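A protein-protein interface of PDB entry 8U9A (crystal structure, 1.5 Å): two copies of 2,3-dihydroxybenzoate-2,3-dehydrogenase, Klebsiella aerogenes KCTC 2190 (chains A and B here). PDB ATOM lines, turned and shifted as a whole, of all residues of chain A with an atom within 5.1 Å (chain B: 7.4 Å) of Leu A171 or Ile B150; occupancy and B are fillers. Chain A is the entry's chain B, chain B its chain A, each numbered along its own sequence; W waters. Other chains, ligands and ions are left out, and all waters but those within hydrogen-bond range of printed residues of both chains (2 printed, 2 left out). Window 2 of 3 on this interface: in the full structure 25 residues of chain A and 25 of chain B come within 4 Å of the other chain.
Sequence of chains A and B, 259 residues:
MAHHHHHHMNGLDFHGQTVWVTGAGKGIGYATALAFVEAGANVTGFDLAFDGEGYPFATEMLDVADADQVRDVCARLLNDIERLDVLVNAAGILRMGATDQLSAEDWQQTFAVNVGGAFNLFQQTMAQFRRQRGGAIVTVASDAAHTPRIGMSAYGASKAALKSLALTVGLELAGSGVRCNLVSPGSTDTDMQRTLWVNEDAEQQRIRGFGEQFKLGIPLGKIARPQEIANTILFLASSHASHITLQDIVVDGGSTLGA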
ATOM      1  N   LEU A 167     -13.816  -1.475  16.710  1.00  0.00           N
ATOM      2  CA  LEU A 167     -15.077  -2.187  16.849  1.00  0.00           C
ATOM      3  C   LEU A 167     -15.764  -2.344  15.499  1.00  0.00           C
ATOM      4  O   LEU A 167     -16.371  -3.377  15.237  1.00  0.00           O
ATOM      5  CB  LEU A 167     -15.999  -1.489  17.858  1.00  0.00           C
ATOM      6  CG  LEU A 167     -15.455  -1.456  19.301  1.00  0.00           C
ATOM      7  CD1 LEU A 167     -16.378  -0.611  20.211  1.00  0.00           C
ATOM      8  CD2 LEU A 167     -15.282  -2.829  19.858  1.00  0.00           C
ATOM      9  N   THR A 168     -15.718  -1.322  14.637  1.00  0.00           N
ATOM     10  CA  THR A 168     -16.367  -1.495  13.339  1.00  0.00           C
ATOM     11  C   THR A 168     -15.609  -2.503  12.481  1.00  0.00           C
ATOM     12  O   THR A 168     -16.232  -3.314  11.786  1.00  0.00           O
ATOM     13  CB  THR A 168     -16.536  -0.150  12.639  1.00  0.00           C
ATOM     14  OG1 THR A 168     -17.342   0.690  13.467  1.00  0.00           O
ATOM     15  CG2 THR A 168     -17.261  -0.337  11.316  1.00  0.00           C
ATOM     16  N   VAL A 169     -14.275  -2.495  12.551  1.00  0.00           N
ATOM     17  CA  VAL A 169     -13.490  -3.526  11.888  1.00  0.00           C
ATOM     18  C   VAL A 169     -13.863  -4.902  12.427  1.00  0.00           C
ATOM     19  O   VAL A 169     -14.014  -5.863  11.664  1.00  0.00           O
ATOM     20  CB  VAL A 169     -11.993  -3.227  12.036  1.00  0.00           C
ATOM     21  CG1 VAL A 169     -11.147  -4.435  11.619  1.00  0.00           C
ATOM     22  CG2 VAL A 169     -11.627  -2.011  11.204  1.00  0.00           C
ATOM     23  N   GLY A 170     -14.068  -5.011  13.740  1.00  0.00           N
ATOM     24  CA  GLY A 170     -14.528  -6.265  14.307  1.00  0.00           C
ATOM     25  C   GLY A 170     -15.859  -6.715  13.751  1.00  0.00           C
ATOM     26  O   GLY A 170     -16.078  -7.903  13.533  1.00  0.00           O
ATOM     27  N   LEU A 171     -16.791  -5.775  13.553  1.00  0.00           N
ATOM     28  CA  LEU A 171     -18.042  -6.132  12.906  1.00  0.00           C
ATOM     29  C   LEU A 171     -17.825  -6.554  11.451  1.00  0.00           C
ATOM     30  O   LEU A 171     -18.422  -7.544  10.989  1.00  0.00           O
ATOM     31  CB  LEU A 171     -18.999  -4.945  13.027  1.00  0.00           C
ATOM     32  CG  LEU A 171     -20.456  -5.157  12.720  1.00  0.00           C
ATOM     33  CD1 LEU A 171     -21.052  -6.293  13.582  1.00  0.00           C
ATOM     34  CD2 LEU A 171     -21.188  -3.830  12.959  1.00  0.00           C
ATOM     35  N   GLU A 172     -16.960  -5.830  10.718  1.00  0.00           N
ATOM     36  CA  GLU A 172     -16.667  -6.179   9.324  1.00  0.00           C
ATOM     37  C   GLU A 172     -16.044  -7.551   9.191  1.00  0.00           C
ATOM     38  O   GLU A 172     -16.250  -8.217   8.175  1.00  0.00           O
ATOM     39  CB  GLU A 172     -15.730  -5.147   8.698  1.00  0.00           C
ATOM     40  CG  GLU A 172     -16.418  -3.823   8.458  1.00  0.00           C
ATOM     41  CD  GLU A 172     -15.456  -2.711   8.009  1.00  0.00           C
ATOM     42  OE1 GLU A 172     -14.498  -2.401   8.751  1.00  0.00           O
ATOM     43  OE2 GLU A 172     -15.659  -2.175   6.913  1.00  0.00           O
ATOM     44  N   LEU A 173     -15.268  -7.990  10.185  1.00  0.00           N
ATOM     45  CA  LEU A 173     -14.573  -9.269  10.100  1.00  0.00           C
ATOM     46  C   LEU A 173     -15.266 -10.382  10.866  1.00  0.00           C
ATOM     47  O   LEU A 173     -14.822 -11.531  10.790  1.00  0.00           O
ATOM     48  CB  LEU A 173     -13.146  -9.108  10.606  1.00  0.00           C
ATOM     49  CG  LEU A 173     -12.217  -8.216   9.765  1.00  0.00           C
ATOM     50  CD1 LEU A 173     -10.865  -8.118  10.413  1.00  0.00           C
ATOM     51  CD2 LEU A 173     -12.081  -8.774   8.369  1.00  0.00           C
ATOM     52  N   ALA A 174     -16.367 -10.096  11.559  1.00  0.00           N
ATOM     53  CA  ALA A 174     -17.038 -11.147  12.324  1.00  0.00           C
ATOM     54  C   ALA A 174     -17.511 -12.280  11.423  1.00  0.00           C
ATOM     55  O   ALA A 174     -17.512 -13.447  11.830  1.00  0.00           O
ATOM     56  CB  ALA A 174     -18.230 -10.572  13.091  1.00  0.00           C
ATOM     57  N   GLY A 175     -17.960 -11.965  10.207  1.00  0.00           N
ATOM     58  CA  GLY A 175     -18.386 -13.015   9.300  1.00  0.00           C
ATOM     59  C   GLY A 175     -17.260 -13.914   8.848  1.00  0.00           C
ATOM     60  O   GLY A 175     -17.516 -15.020   8.356  1.00  0.00           O
ATOM     61  N   LEU A 246     -15.634  -7.697  20.386  1.00  0.00           N
ATOM     62  CA  LEU A 246     -16.084  -6.300  20.472  1.00  0.00           C
ATOM     63  C   LEU A 246     -16.073  -5.806  21.909  1.00  0.00           C
ATOM     64  O   LEU A 246     -16.812  -4.883  22.245  1.00  0.00           O
ATOM     65  CB  LEU A 246     -17.462  -6.085  19.832  1.00  0.00           C
ATOM     66  CG  LEU A 246     -17.643  -6.716  18.452  1.00  0.00           C
ATOM     67  CD1 LEU A 246     -19.034  -6.419  17.883  1.00  0.00           C
ATOM     68  CD2 LEU A 246     -16.569  -6.294  17.482  1.00  0.00           C
ATOM     69  N   MET B  96     -18.395   7.026   3.067  1.00  0.00           N
ATOM     70  CA  MET B  96     -18.610   5.642   3.440  1.00  0.00           C
ATOM     71  C   MET B  96     -17.705   4.726   2.651  1.00  0.00           C
ATOM     72  O   MET B  96     -17.127   5.099   1.630  1.00  0.00           O
ATOM     73  CB  MET B  96     -20.074   5.259   3.241  1.00  0.00           C
ATOM     74  CG  MET B  96     -20.954   5.981   4.243  1.00  0.00           C
ATOM     75  SD  MET B  96     -22.687   5.590   4.091  1.00  0.00           S
ATOM     76  CE  MET B  96     -22.998   6.068   2.398  1.00  0.00           C
ATOM     77  N   GLY B  97     -17.554   3.516   3.174  1.00  0.00           N
ATOM     78  CA  GLY B  97     -16.775   2.482   2.534  1.00  0.00           C
ATOM     79  C   GLY B  97     -16.336   1.416   3.514  1.00  0.00           C
ATOM     80  O   GLY B  97     -16.214   1.692   4.711  1.00  0.00           O
ATOM     81  N   ALA B  98     -16.095   0.214   3.010  1.00  0.00           N
ATOM     82  CA  ALA B  98     -15.389  -0.804   3.772  1.00  0.00           C
ATOM     83  C   ALA B  98     -14.055  -0.234   4.220  1.00  0.00           C
ATOM     84  O   ALA B  98     -13.426   0.544   3.498  1.00  0.00           O
ATOM     85  CB  ALA B  98     -15.165  -2.055   2.928  1.00  0.00           C
ATOM     86  N   THR B 147     -22.339   3.017  18.216  1.00  0.00           N
ATOM     87  CA  THR B 147     -22.456   1.617  17.906  1.00  0.00           C
ATOM     88  C   THR B 147     -21.718   1.453  16.586  1.00  0.00           C
ATOM     89  O   THR B 147     -21.763   2.361  15.755  1.00  0.00           O
ATOM     90  CB  THR B 147     -23.922   1.173  17.787  1.00  0.00           C
ATOM     91  OG1 THR B 147     -23.990  -0.246  17.653  1.00  0.00           O
ATOM     92  CG2 THR B 147     -24.586   1.810  16.577  1.00  0.00           C
ATOM     93  N   PRO B 148     -21.032   0.340  16.361  1.00  0.00           N
ATOM     94  CA  PRO B 148     -20.346   0.163  15.077  1.00  0.00           C
ATOM     95  C   PRO B 148     -21.331  -0.028  13.939  1.00  0.00           C
ATOM     96  O   PRO B 148     -22.331  -0.732  14.070  1.00  0.00           O
ATOM     97  CB  PRO B 148     -19.508  -1.101  15.295  1.00  0.00           C
ATOM     98  CG  PRO B 148     -20.167  -1.811  16.421  1.00  0.00           C
ATOM     99  CD  PRO B 148     -20.751  -0.762  17.298  1.00  0.00           C
ATOM    100  N   ARG B 149     -21.047   0.632  12.820  1.00  0.00           N
ATOM    101  CA  ARG B 149     -21.918   0.595  11.653  1.00  0.00           C
ATOM    102  C   ARG B 149     -21.092   0.219  10.434  1.00  0.00           C
ATOM    103  O   ARG B 149     -20.166   0.949  10.073  1.00  0.00           O
ATOM    104  CB  ARG B 149     -22.582   1.954  11.451  1.00  0.00           C
ATOM    105  CG  ARG B 149     -23.515   2.335  12.598  1.00  0.00           C
ATOM    106  CD  ARG B 149     -24.864   1.668  12.451  1.00  0.00           C
ATOM    107  NE  ARG B 149     -25.580   2.213  11.304  1.00  0.00           N
ATOM    108  CZ  ARG B 149     -26.229   3.370  11.306  1.00  0.00           C
ATOM    109  NH1 ARG B 149     -26.317   4.114  12.398  1.00  0.00           N
ATOM    110  NH2 ARG B 149     -26.798   3.795  10.181  1.00  0.00           N
ATOM    111  N   ILE B 150     -21.456  -0.894   9.786  1.00  0.00           N
ATOM    112  CA  ILE B 150     -20.770  -1.312   8.570  1.00  0.00           C
ATOM    113  C   ILE B 150     -20.826  -0.189   7.543  1.00  0.00           C
ATOM    114  O   ILE B 150     -21.862   0.445   7.347  1.00  0.00           O
ATOM    115  CB  ILE B 150     -21.395  -2.592   7.994  1.00  0.00           C
ATOM    116  CG1 ILE B 150     -21.335  -3.735   9.004  1.00  0.00           C
ATOM    117  CG2 ILE B 150     -20.643  -3.006   6.717  1.00  0.00           C
ATOM    118  CD1 ILE B 150     -19.995  -4.360   9.098  1.00  0.00           C
ATOM    119  N   GLY B 151     -19.696   0.056   6.878  1.00  0.00           N
ATOM    120  CA  GLY B 151     -19.588   1.117   5.909  1.00  0.00           C
ATOM    121  C   GLY B 151     -19.236   2.459   6.484  1.00  0.00           C
ATOM    122  O   GLY B 151     -18.962   3.389   5.718  1.00  0.00           O
ATOM    123  N   MET B 152     -19.256   2.605   7.805  1.00  0.00           N
ATOM    124  CA  MET B 152     -19.082   3.901   8.436  1.00  0.00           C
ATOM    125  C   MET B 152     -17.934   3.885   9.434  1.00  0.00           C
ATOM    126  O   MET B 152     -17.929   4.658  10.391  1.00  0.00           O
ATOM    127  CB  MET B 152     -20.377   4.344   9.118  1.00  0.00           C
ATOM    128  CG  MET B 152     -21.424   4.796   8.140  1.00  0.00           C
ATOM    129  SD  MET B 152     -22.924   5.300   9.001  1.00  0.00           S
ATOM    130  CE  MET B 152     -23.846   5.949   7.609  1.00  0.00           C
ATOM    131  N   SER B 153     -16.930   3.030   9.234  1.00  0.00           N
ATOM    132  CA  SER B 153     -15.875   2.922  10.233  1.00  0.00           C
ATOM    133  C   SER B 153     -15.161   4.255  10.441  1.00  0.00           C
ATOM    134  O   SER B 153     -14.978   4.699  11.583  1.00  0.00           O
ATOM    135  CB  SER B 153     -14.894   1.823   9.848  1.00  0.00           C
ATOM    136  OG  SER B 153     -14.189   2.191   8.682  1.00  0.00           O
HETATM  137  O   HOH W   1     -16.662   3.372  13.588  1.00  0.00           O
HETATM  138  O   HOH W   2     -19.612   3.226  13.312  1.00  0.00           O
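Among the printed residues, merely in contact across the chains: Leu A167 with Pro B148, Thr A168 with Pro B148, Thr A168 with Arg B149, Thr A168 with Ser B153, Leu A171 with Pro B148, Leu A171 with Ile B150, Glu A172 with Ala B98 and Glu A172 with Ile B150.
Leu A171 touches just these residues of chain B: Pro B148 (3.5 Å) and Ile B150 (3.7 Å).
Of the printed residues of chain A, Ile B150 touches Leu A171 (3.7 Å) and Glu A172 (3.7 Å).
Of the printed residues of chain A, Arg B149 touches Thr A168.
Of the printed residues of chain B, Thr A168 touches Pro B148, Arg B149 and Ser B153.
Met B152 touches none of the printed residues of chain A.
Val A169 touches none of the printed residues of chain B.
Hydrophobic or aromatic side chains of chain B that line the printed part of chain A: Pro B148 and Ile B150.
Of the 10 printed residues of chain A, 4 touch a printed residue of chain B.
Printed residues of chain A that touch a printed residue of chain B: Leu A167, Thr A168, Leu A171 and Glu A172.
Hydrophobic or aromatic side chains of chain A that line the printed part of chain B: Leu A171.
Among the printed residues, no Asp or Glu carboxylate lies within 4 Å of a Lys or Arg side-chain nitrogen of the other chain.
No position is printed for both chains.
Water W1 bridges OG1 of Thr A168 and O of Ser B153.
Water W2 lies within hydrogen-bond range of the backbone NH of Arg B149 (3.0 Å), the backbone carbonyl oxygen of Thr B147 (3.4 Å) and the side-chain hydroxyl of Thr A168 (3.4 Å).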
